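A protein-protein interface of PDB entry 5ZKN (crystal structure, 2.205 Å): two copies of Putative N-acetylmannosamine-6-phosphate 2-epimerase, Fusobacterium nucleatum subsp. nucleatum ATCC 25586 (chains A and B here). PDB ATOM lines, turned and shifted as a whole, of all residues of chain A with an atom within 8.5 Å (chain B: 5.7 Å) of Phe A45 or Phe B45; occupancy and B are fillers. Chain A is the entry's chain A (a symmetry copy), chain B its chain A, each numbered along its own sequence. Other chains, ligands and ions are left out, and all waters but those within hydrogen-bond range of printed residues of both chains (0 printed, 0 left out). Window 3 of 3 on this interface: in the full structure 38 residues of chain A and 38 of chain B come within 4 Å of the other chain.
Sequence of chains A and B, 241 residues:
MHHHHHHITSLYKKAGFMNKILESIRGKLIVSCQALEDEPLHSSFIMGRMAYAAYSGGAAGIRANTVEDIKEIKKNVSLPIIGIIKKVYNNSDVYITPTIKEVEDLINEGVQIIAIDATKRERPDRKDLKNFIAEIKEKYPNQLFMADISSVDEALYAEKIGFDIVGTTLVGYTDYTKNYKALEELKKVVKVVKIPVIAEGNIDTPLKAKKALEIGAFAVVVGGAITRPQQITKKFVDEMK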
ATOM      1  N   PRO A  40       8.246   8.367   6.713  1.00  0.00           N
ATOM      2  CA  PRO A  40       7.908   7.997   8.100  1.00  0.00           C
ATOM      3  C   PRO A  40       8.551   8.833   9.193  1.00  0.00           C
ATOM      4  O   PRO A  40       7.864   9.198  10.158  1.00  0.00           O
ATOM      5  CB  PRO A  40       8.371   6.536   8.166  1.00  0.00           C
ATOM      6  CG  PRO A  40       8.120   6.021   6.781  1.00  0.00           C
ATOM      7  CD  PRO A  40       8.521   7.181   5.881  1.00  0.00           C
ATOM      8  N   LEU A  41       9.851   9.121   9.106  1.00  0.00           N
ATOM      9  CA  LEU A  41      10.557   9.797  10.191  1.00  0.00           C
ATOM     10  C   LEU A  41      10.783  11.277   9.930  1.00  0.00           C
ATOM     11  O   LEU A  41      11.681  11.859  10.541  1.00  0.00           O
ATOM     12  CB  LEU A  41      11.916   9.142  10.468  1.00  0.00           C
ATOM     13  CG  LEU A  41      11.923   7.625  10.458  1.00  0.00           C
ATOM     14  CD1 LEU A  41      13.404   7.209  10.483  1.00  0.00           C
ATOM     15  CD2 LEU A  41      11.089   7.027  11.636  1.00  0.00           C
ATOM     16  N   HIS A  42       9.997  11.899   9.054  1.00  0.00           N
ATOM     17  CA  HIS A  42      10.115  13.334   8.840  1.00  0.00           C
ATOM     18  C   HIS A  42       9.912  14.079  10.148  1.00  0.00           C
ATOM     19  O   HIS A  42       8.816  14.050  10.718  1.00  0.00           O
ATOM     20  CB  HIS A  42       9.114  13.828   7.796  1.00  0.00           C
ATOM     21  CG  HIS A  42       9.098  15.316   7.633  1.00  0.00           C
ATOM     22  ND1 HIS A  42      10.086  15.998   6.953  1.00  0.00           N
ATOM     23  CD2 HIS A  42       8.184  16.248   8.003  1.00  0.00           C
ATOM     24  CE1 HIS A  42       9.791  17.288   6.941  1.00  0.00           C
ATOM     25  NE2 HIS A  42       8.640  17.466   7.566  1.00  0.00           N
ATOM     26  N   SER A  43      10.980  14.724  10.626  1.00  0.00           N
ATOM     27  CA  SER A  43      11.037  15.420  11.908  1.00  0.00           C
ATOM     28  C   SER A  43      12.479  15.834  12.161  1.00  0.00           C
ATOM     29  O   SER A  43      13.383  14.989  12.117  1.00  0.00           O
ATOM     30  CB  SER A  43      10.542  14.539  13.056  1.00  0.00           C
ATOM     31  OG  SER A  43      11.130  14.959  14.278  1.00  0.00           O
ATOM     32  N   SER A  44      12.707  17.122  12.420  1.00  0.00           N
ATOM     33  CA  SER A  44      14.063  17.575  12.715  1.00  0.00           C
ATOM     34  C   SER A  44      14.607  16.884  13.958  1.00  0.00           C
ATOM     35  O   SER A  44      15.784  16.502  13.999  1.00  0.00           O
ATOM     36  CB  SER A  44      14.088  19.097  12.881  1.00  0.00           C
ATOM     37  OG  SER A  44      13.773  19.756  11.664  1.00  0.00           O
ATOM     38  N   PHE A  45      13.756  16.696  14.977  1.00  0.00           N
ATOM     39  CA  PHE A  45      14.169  15.975  16.179  1.00  0.00           C
ATOM     40  C   PHE A  45      14.770  14.604  15.853  1.00  0.00           C
ATOM     41  O   PHE A  45      15.864  14.260  16.325  1.00  0.00           O
ATOM     42  CB  PHE A  45      12.986  15.807  17.122  1.00  0.00           C
ATOM     43  CG  PHE A  45      13.306  14.969  18.323  1.00  0.00           C
ATOM     44  CD1 PHE A  45      14.461  15.207  19.059  1.00  0.00           C
ATOM     45  CD2 PHE A  45      12.473  13.935  18.717  1.00  0.00           C
ATOM     46  CE1 PHE A  45      14.779  14.432  20.173  1.00  0.00           C
ATOM     47  CE2 PHE A  45      12.785  13.160  19.833  1.00  0.00           C
ATOM     48  CZ  PHE A  45      13.952  13.405  20.552  1.00  0.00           C
ATOM     49  N   ILE A  46      14.057  13.806  15.055  1.00  0.00           N
ATOM     50  CA  ILE A  46      14.510  12.449  14.738  1.00  0.00           C
ATOM     51  C   ILE A  46      15.801  12.478  13.922  1.00  0.00           C
ATOM     52  O   ILE A  46      16.688  11.625  14.093  1.00  0.00           O
ATOM     53  CB  ILE A  46      13.407  11.658  13.995  1.00  0.00           C
ATOM     54  CG1 ILE A  46      12.124  11.600  14.835  1.00  0.00           C
ATOM     55  CG2 ILE A  46      13.921  10.256  13.626  1.00  0.00           C
ATOM     56  CD1 ILE A  46      11.103  10.594  14.365  1.00  0.00           C
ATOM     57  N   MET A  47      15.911  13.421  12.991  1.00  0.00           N
ATOM     58  CA  MET A  47      17.109  13.465  12.164  1.00  0.00           C
ATOM     59  C   MET A  47      18.328  13.839  13.014  1.00  0.00           C
ATOM     60  O   MET A  47      19.438  13.341  12.776  1.00  0.00           O
ATOM     61  CB  MET A  47      16.880  14.447  11.010  1.00  0.00           C
ATOM     62  CG  MET A  47      15.847  13.948  10.008  1.00  0.00           C
ATOM     63  SD  MET A  47      16.323  12.367   9.196  1.00  0.00           S
ATOM     64  CE  MET A  47      15.260  11.170  10.054  1.00  0.00           C
ATOM     65  N   GLY A  48      18.125  14.696  14.021  1.00  0.00           N
ATOM     66  CA  GLY A  48      19.171  14.937  14.998  1.00  0.00           C
ATOM     67  C   GLY A  48      19.593  13.665  15.713  1.00  0.00           C
ATOM     68  O   GLY A  48      20.788  13.395  15.868  1.00  0.00           O
ATOM     69  N   ARG A  49      18.624  12.851  16.140  1.00  0.00           N
ATOM     70  CA  ARG A  49      19.010  11.626  16.834  1.00  0.00           C
ATOM     71  C   ARG A  49      19.622  10.611  15.877  1.00  0.00           C
ATOM     72  O   ARG A  49      20.542   9.870  16.266  1.00  0.00           O
ATOM     73  CB  ARG A  49      17.820  11.040  17.585  1.00  0.00           C
ATOM     74  CG  ARG A  49      17.336  11.912  18.746  1.00  0.00           C
ATOM     75  CD  ARG A  49      18.305  11.908  19.928  1.00  0.00           C
ATOM     76  NE  ARG A  49      17.725  12.496  21.132  1.00  0.00           N
ATOM     77  CZ  ARG A  49      17.063  11.781  22.041  1.00  0.00           C
ATOM     78  NH1 ARG A  49      16.911  10.469  21.858  1.00  0.00           N
ATOM     79  NH2 ARG A  49      16.536  12.363  23.115  1.00  0.00           N
ATOM     80  N   MET A  50      19.159  10.574  14.617  1.00  0.00           N
ATOM     81  CA  MET A  50      19.810   9.705  13.631  1.00  0.00           C
ATOM     82  C   MET A  50      21.277  10.093  13.449  1.00  0.00           C
ATOM     83  O   MET A  50      22.147   9.222  13.356  1.00  0.00           O
ATOM     84  CB  MET A  50      19.088   9.763  12.282  1.00  0.00           C
ATOM     85  CG  MET A  50      17.746   9.027  12.227  1.00  0.00           C
ATOM     86  SD  MET A  50      17.967   7.244  12.067  1.00  0.00           S
ATOM     87  CE  MET A  50      16.748   6.782  13.255  1.00  0.00           C
ATOM     88  N   ALA A  51      21.561  11.397  13.369  1.00  0.00           N
ATOM     89  CA  ALA A  51      22.951  11.856  13.289  1.00  0.00           C
ATOM     90  C   ALA A  51      23.747  11.374  14.491  1.00  0.00           C
ATOM     91  O   ALA A  51      24.860  10.867  14.356  1.00  0.00           O
ATOM     92  CB  ALA A  51      22.998  13.381  13.203  1.00  0.00           C
ATOM     93  N   TYR A  52      23.178  11.520  15.689  1.00  0.00           N
ATOM     94  CA  TYR A  52      23.856  11.021  16.879  1.00  0.00           C
ATOM     95  C   TYR A  52      24.121   9.515  16.796  1.00  0.00           C
ATOM     96  O   TYR A  52      25.173   9.036  17.236  1.00  0.00           O
ATOM     97  CB  TYR A  52      23.045  11.360  18.125  1.00  0.00           C
ATOM     98  CG  TYR A  52      23.839  10.986  19.354  1.00  0.00           C
ATOM     99  CD1 TYR A  52      23.411   9.988  20.220  1.00  0.00           C
ATOM    100  CD2 TYR A  52      25.080  11.572  19.594  1.00  0.00           C
ATOM    101  CE1 TYR A  52      24.166   9.631  21.329  1.00  0.00           C
ATOM    102  CE2 TYR A  52      25.847  11.212  20.687  1.00  0.00           C
ATOM    103  CZ  TYR A  52      25.383  10.236  21.558  1.00  0.00           C
ATOM    104  OH  TYR A  52      26.134   9.856  22.659  1.00  0.00           O
ATOM    105  N   GLU A  68      16.149  23.525   9.261  1.00  0.00           N
ATOM    106  CA  GLU A  68      15.634  23.041  10.539  1.00  0.00           C
ATOM    107  C   GLU A  68      16.247  21.693  10.923  1.00  0.00           C
ATOM    108  O   GLU A  68      16.527  21.455  12.103  1.00  0.00           O
ATOM    109  CB  GLU A  68      14.107  22.972  10.512  1.00  0.00           C
ATOM    110  CG  GLU A  68      13.488  22.430   9.241  1.00  0.00           C
ATOM    111  CD  GLU A  68      11.960  22.447   9.301  1.00  0.00           C
ATOM    112  OE1 GLU A  68      11.397  22.285  10.411  1.00  0.00           O
ATOM    113  OE2 GLU A  68      11.324  22.633   8.240  1.00  0.00           O
ATOM    114  N   ASP A  69      16.499  20.810   9.945  1.00  0.00           N
ATOM    115  CA  ASP A  69      17.191  19.551  10.249  1.00  0.00           C
ATOM    116  C   ASP A  69      18.661  19.794  10.609  1.00  0.00           C
ATOM    117  O   ASP A  69      19.183  19.217  11.571  1.00  0.00           O
ATOM    118  CB  ASP A  69      17.110  18.587   9.064  1.00  0.00           C
ATOM    119  CG  ASP A  69      15.735  17.914   8.909  1.00  0.00           C
ATOM    120  OD1 ASP A  69      14.737  18.363   9.525  1.00  0.00           O
ATOM    121  OD2 ASP A  69      15.669  16.921   8.138  1.00  0.00           O
ATOM    122  N   LYS A  71      20.099  22.463  11.850  1.00  0.00           N
ATOM    123  CA  LYS A  71      20.164  23.063  13.186  1.00  0.00           C
ATOM    124  C   LYS A  71      20.069  22.004  14.275  1.00  0.00           C
ATOM    125  O   LYS A  71      20.894  21.962  15.194  1.00  0.00           O
ATOM    126  CB  LYS A  71      19.033  24.080  13.365  1.00  0.00           C
ATOM    127  CG  LYS A  71      19.208  25.342  12.574  1.00  0.00           C
ATOM    128  CD  LYS A  71      17.946  26.179  12.555  1.00  0.00           C
ATOM    129  CE  LYS A  71      17.704  26.827  13.893  1.00  0.00           C
ATOM    130  NZ  LYS A  71      16.435  27.611  13.863  1.00  0.00           N
ATOM    131  N   GLU A  72      19.041  21.156  14.197  1.00  0.00           N
ATOM    132  CA  GLU A  72      18.866  20.104  15.187  1.00  0.00           C
ATOM    133  C   GLU A  72      20.057  19.148  15.189  1.00  0.00           C
ATOM    134  O   GLU A  72      20.516  18.720  16.255  1.00  0.00           O
ATOM    135  CB  GLU A  72      17.556  19.361  14.906  1.00  0.00           C
ATOM    136  CG  GLU A  72      17.150  18.406  15.991  1.00  0.00           C
ATOM    137  CD  GLU A  72      16.628  19.105  17.241  1.00  0.00           C
ATOM    138  OE1 GLU A  72      16.060  20.228  17.141  1.00  0.00           O
ATOM    139  OE2 GLU A  72      16.792  18.514  18.329  1.00  0.00           O
ATOM    140  N   ILE A  73      20.576  18.808  14.005  1.00  0.00           N
ATOM    141  CA  ILE A  73      21.748  17.933  13.923  1.00  0.00           C
ATOM    142  C   ILE A  73      22.950  18.559  14.623  1.00  0.00           C
ATOM    143  O   ILE A  73      23.729  17.864  15.294  1.00  0.00           O
ATOM    144  CB  ILE A  73      22.040  17.594  12.453  1.00  0.00           C
ATOM    145  CG1 ILE A  73      20.908  16.699  11.941  1.00  0.00           C
ATOM    146  CG2 ILE A  73      23.418  16.920  12.290  1.00  0.00           C
ATOM    147  CD1 ILE A  73      21.061  16.285  10.537  1.00  0.00           C
ATOM    148  N   LYS A  75      22.938  20.291  17.244  1.00  0.00           N
ATOM    149  CA  LYS A  75      22.779  20.136  18.687  1.00  0.00           C
ATOM    150  C   LYS A  75      23.260  18.783  19.180  1.00  0.00           C
ATOM    151  O   LYS A  75      23.578  18.651  20.369  1.00  0.00           O
ATOM    152  CB  LYS A  75      21.309  20.294  19.089  1.00  0.00           C
ATOM    153  CG  LYS A  75      20.656  21.608  18.704  1.00  0.00           C
ATOM    154  CD  LYS A  75      19.254  21.623  19.267  1.00  0.00           C
ATOM    155  CE  LYS A  75      18.561  22.925  19.009  1.00  0.00           C
ATOM    156  NZ  LYS A  75      17.114  22.798  19.366  1.00  0.00           N
ATOM    157  N   ASN A  76      23.312  17.782  18.291  1.00  0.00           N
ATOM    158  CA  ASN A  76      23.596  16.397  18.638  1.00  0.00           C
ATOM    159  C   ASN A  76      25.033  15.971  18.353  1.00  0.00           C
ATOM    160  O   ASN A  76      25.589  15.161  19.103  1.00  0.00           O
ATOM    161  CB  ASN A  76      22.623  15.465  17.888  1.00  0.00           C
ATOM    162  CG  ASN A  76      21.240  15.485  18.506  1.00  0.00           C
ATOM    163  OD1 ASN A  76      20.948  14.699  19.419  1.00  0.00           O
ATOM    164  ND2 ASN A  76      20.405  16.437  18.077  1.00  0.00           N
ATOM    165  N   HIS B  42      16.437   6.621  22.023  1.00  0.00           N
ATOM    166  CA  HIS B  42      15.530   6.472  23.153  1.00  0.00           C
ATOM    167  C   HIS B  42      14.560   7.639  23.205  1.00  0.00           C
ATOM    168  O   HIS B  42      14.973   8.784  23.428  1.00  0.00           O
ATOM    169  CB  HIS B  42      16.293   6.366  24.472  1.00  0.00           C
ATOM    170  CG  HIS B  42      15.409   6.347  25.680  1.00  0.00           C
ATOM    171  ND1 HIS B  42      14.686   5.232  26.052  1.00  0.00           N
ATOM    172  CD2 HIS B  42      15.179   7.281  26.638  1.00  0.00           C
ATOM    173  CE1 HIS B  42      14.029   5.496  27.170  1.00  0.00           C
ATOM    174  NE2 HIS B  42      14.314   6.729  27.549  1.00  0.00           N
ATOM    175  N   SER B  43      13.277   7.347  22.977  1.00  0.00           N
ATOM    176  CA  SER B  43      12.195   8.322  22.884  1.00  0.00           C
ATOM    177  C   SER B  43      10.942   7.599  22.412  1.00  0.00           C
ATOM    178  O   SER B  43      10.970   6.924  21.375  1.00  0.00           O
ATOM    179  CB  SER B  43      12.534   9.458  21.917  1.00  0.00           C
ATOM    180  OG  SER B  43      11.342  10.024  21.397  1.00  0.00           O
ATOM    181  N   SER B  44       9.846   7.728  23.160  1.00  0.00           N
ATOM    182  CA  SER B  44       8.600   7.096  22.738  1.00  0.00           C
ATOM    183  C   SER B  44       8.147   7.638  21.389  1.00  0.00           C
ATOM    184  O   SER B  44       7.670   6.878  20.536  1.00  0.00           O
ATOM    185  CB  SER B  44       7.516   7.301  23.800  1.00  0.00           C
ATOM    186  OG  SER B  44       7.840   6.626  25.007  1.00  0.00           O
ATOM    187  N   PHE B  45       8.309   8.950  21.170  1.00  0.00           N
ATOM    188  CA  PHE B  45       7.973   9.545  19.878  1.00  0.00           C
ATOM    189  C   PHE B  45       8.657   8.821  18.714  1.00  0.00           C
ATOM    190  O   PHE B  45       8.005   8.443  17.729  1.00  0.00           O
ATOM    191  CB  PHE B  45       8.356  11.019  19.864  1.00  0.00           C
ATOM    192  CG  PHE B  45       8.153  11.665  18.527  1.00  0.00           C
ATOM    193  CD1 PHE B  45       6.964  11.484  17.832  1.00  0.00           C
ATOM    194  CD2 PHE B  45       9.145  12.441  17.950  1.00  0.00           C
ATOM    195  CE1 PHE B  45       6.761  12.071  16.583  1.00  0.00           C
ATOM    196  CE2 PHE B  45       8.945  13.033  16.702  1.00  0.00           C
ATOM    197  CZ  PHE B  45       7.751  12.831  16.015  1.00  0.00           C
ATOM    198  N   ILE B  46       9.974   8.632  18.810  1.00  0.00           N
ATOM    199  CA  ILE B  46      10.733   8.012  17.720  1.00  0.00           C
ATOM    200  C   ILE B  46      10.317   6.556  17.521  1.00  0.00           C
ATOM    201  O   ILE B  46      10.262   6.054  16.386  1.00  0.00           O
ATOM    202  CB  ILE B  46      12.255   8.119  17.977  1.00  0.00           C
ATOM    203  CG1 ILE B  46      12.675   9.586  18.140  1.00  0.00           C
ATOM    204  CG2 ILE B  46      13.031   7.418  16.850  1.00  0.00           C
ATOM    205  CD1 ILE B  46      14.161   9.833  18.070  1.00  0.00           C
ATOM    206  N   MET B  47      10.069   5.839  18.613  1.00  0.00           N
ATOM    207  CA  MET B  47       9.704   4.436  18.473  1.00  0.00           C
ATOM    208  C   MET B  47       8.334   4.308  17.799  1.00  0.00           C
ATOM    209  O   MET B  47       8.102   3.374  17.017  1.00  0.00           O
ATOM    210  CB  MET B  47       9.736   3.775  19.856  1.00  0.00           C
ATOM    211  CG  MET B  47      11.147   3.659  20.420  1.00  0.00           C
ATOM    212  SD  MET B  47      12.267   2.636  19.380  1.00  0.00           S
ATOM    213  CE  MET B  47      13.288   3.902  18.571  1.00  0.00           C
ATOM    214  N   GLY B  48       7.431   5.255  18.075  1.00  0.00           N
ATOM    215  CA  GLY B  48       6.193   5.328  17.320  1.00  0.00           C
ATOM    216  C   GLY B  48       6.437   5.513  15.834  1.00  0.00           C
ATOM    217  O   GLY B  48       5.823   4.835  15.004  1.00  0.00           O
ATOM    218  N   ARG B  49       7.351   6.416  15.470  1.00  0.00           N
ATOM    219  CA  ARG B  49       7.596   6.614  14.044  1.00  0.00           C
ATOM    220  C   ARG B  49       8.333   5.428  13.435  1.00  0.00           C
ATOM    221  O   ARG B  49       8.083   5.076  12.269  1.00  0.00           O
ATOM    222  CB  ARG B  49       8.344   7.920  13.805  1.00  0.00           C
ATOM    223  CG  ARG B  49       7.528   9.167  14.152  1.00  0.00           C
ATOM    224  CD  ARG B  49       6.401   9.429  13.154  1.00  0.00           C
ATOM    225  NE  ARG B  49       5.808  10.754  13.310  1.00  0.00           N
ATOM    226  CZ  ARG B  49       6.251  11.828  12.657  1.00  0.00           C
ATOM    227  NH1 ARG B  49       7.282  11.706  11.820  1.00  0.00           N
ATOM    228  NH2 ARG B  49       5.690  13.020  12.845  1.00  0.00           N
ATOM    229  N   MET B  50       9.219   4.774  14.204  1.00  0.00           N
ATOM    230  CA  MET B  50       9.851   3.550  13.701  1.00  0.00           C
ATOM    231  C   MET B  50       8.802   2.481  13.399  1.00  0.00           C
ATOM    232  O   MET B  50       8.890   1.789  12.380  1.00  0.00           O
ATOM    233  CB  MET B  50      10.872   3.005  14.703  1.00  0.00           C
ATOM    234  CG  MET B  50      12.183   3.790  14.795  1.00  0.00           C
ATOM    235  SD  MET B  50      13.287   3.413  13.418  1.00  0.00           S
ATOM    236  CE  MET B  50      13.769   5.077  13.085  1.00  0.00           C
ATOM    237  N   GLU B  72       2.591   5.197  22.453  1.00  0.00           N
ATOM    238  CA  GLU B  72       2.922   5.994  21.281  1.00  0.00           C
ATOM    239  C   GLU B  72       2.829   5.160  20.005  1.00  0.00           C
ATOM    240  O   GLU B  72       2.337   5.640  18.977  1.00  0.00           O
ATOM    241  CB  GLU B  72       4.323   6.588  21.457  1.00  0.00           C
ATOM    242  CG  GLU B  72       4.686   7.613  20.421  1.00  0.00           C
ATOM    243  CD  GLU B  72       3.965   8.942  20.614  1.00  0.00           C
ATOM    244  OE1 GLU B  72       3.620   9.307  21.772  1.00  0.00           O
ATOM    245  OE2 GLU B  72       3.747   9.620  19.588  1.00  0.00           O
ATOM    246  N   ASN B  76       0.327   5.298  16.031  1.00  0.00           N
ATOM    247  CA  ASN B  76       0.897   5.288  14.691  1.00  0.00           C
ATOM    248  C   ASN B  76       0.444   4.110  13.835  1.00  0.00           C
ATOM    249  O   ASN B  76       0.290   4.264  12.619  1.00  0.00           O
ATOM    250  CB  ASN B  76       2.436   5.297  14.785  1.00  0.00           C
ATOM    251  CG  ASN B  76       2.968   6.666  15.155  1.00  0.00           C
ATOM    252  OD1 ASN B  76       3.232   7.497  14.274  1.00  0.00           O
ATOM    253  ND2 ASN B  76       3.048   6.946  16.460  1.00  0.00           N
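Among the printed residues, merely in contact across the chains: Leu A41 with Met B50 (3.4 Å), Met A50 with Met B50 (3.4 Å), Leu A41 with Arg B49 (3.6 Å), Phe A45 with Phe B45 (3.7 Å), Ser A43 with Phe B45 (3.8 Å), Phe A45 with Ser B43 (3.8 Å), Arg A49 with Ile B46 (3.9 Å), Ile A46 with Arg B49 (3.9 Å), Ile A46 with Ile B46 (3.9 Å), Ile A46 with Phe B45 (3.96 Å) and Phe A45 with Ile B46 (3.96 Å).
The side-chain hydroxyl of Ser A43 sits at hydrogen-bond distance from the backbone NH of Ile A46, at 3.2 Å.
OG of Ser B43 sits close to N of Phe B45, at 3.2 Å.
OG of Ser B43 sits at hydrogen-bond distance from N of Ile B46 (3.2 Å).
The backbone NH of Phe A45 lies close to the side-chain hydroxyl of Ser A43, at 3.2 Å.
Phe A45 touches three residues of chain B.
Of chain A, only Ser A43, Phe A45 and Ile A46 come within 4 Å of Phe B45.
Of the printed residues of chain A, Met B50 touches Leu A41 (3.4 Å) and Met A50 (3.4 Å).
Printed residues of chain B within 4 Å of Ile A46: Phe B45 (3.96 Å), Ile B46 (3.9 Å) and Arg B49 (3.9 Å).
Printed residues of chain B within 4 Å of Met A50: Met B50.
Of the printed residues of chain A, His B42 touches Arg A49 (3.0 Å).
Printed residues of chain B within 4 Å of His A42: Arg B49 (3.0 Å).
The nearest printed residue of chain A that does not touch His B42 is Phe A45 (5.5 Å).
Phe A45 touches its own counterpart, Phe B45.
Ile A46 touches its own counterpart, Ile B46.
Ile A46 touches Arg B49, and with the chains exchanged Arg A49 touches Ile B46.
Met B50 touches its own counterpart, Met A50.
Hydrophobic or aromatic side chains of chain B that line the printed part of chain A: Phe B45, Ile B46 and Met B50.
Among the printed residues, 14 pairs touch across the chains.
Among the printed residues, no Asp or Glu carboxylate lies within 4 Å of a Lys or Arg side-chain nitrogen of the other chain.
The backbone carbonyl oxygen (O) of His B42 is in hydrogen-bond range of the guanidinium group (NH1) of Arg A49 (3.0 Å).
The backbone carbonyl oxygen of Pro A40 is in hydrogen-bond range of the guanidinium group of Arg B49 (3.1 Å).
The backbone carbonyl oxygen (O) of His A42 lies within hydrogen-bond range of the guanidinium group (NH1) of Arg B49, 3.0 Å away.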
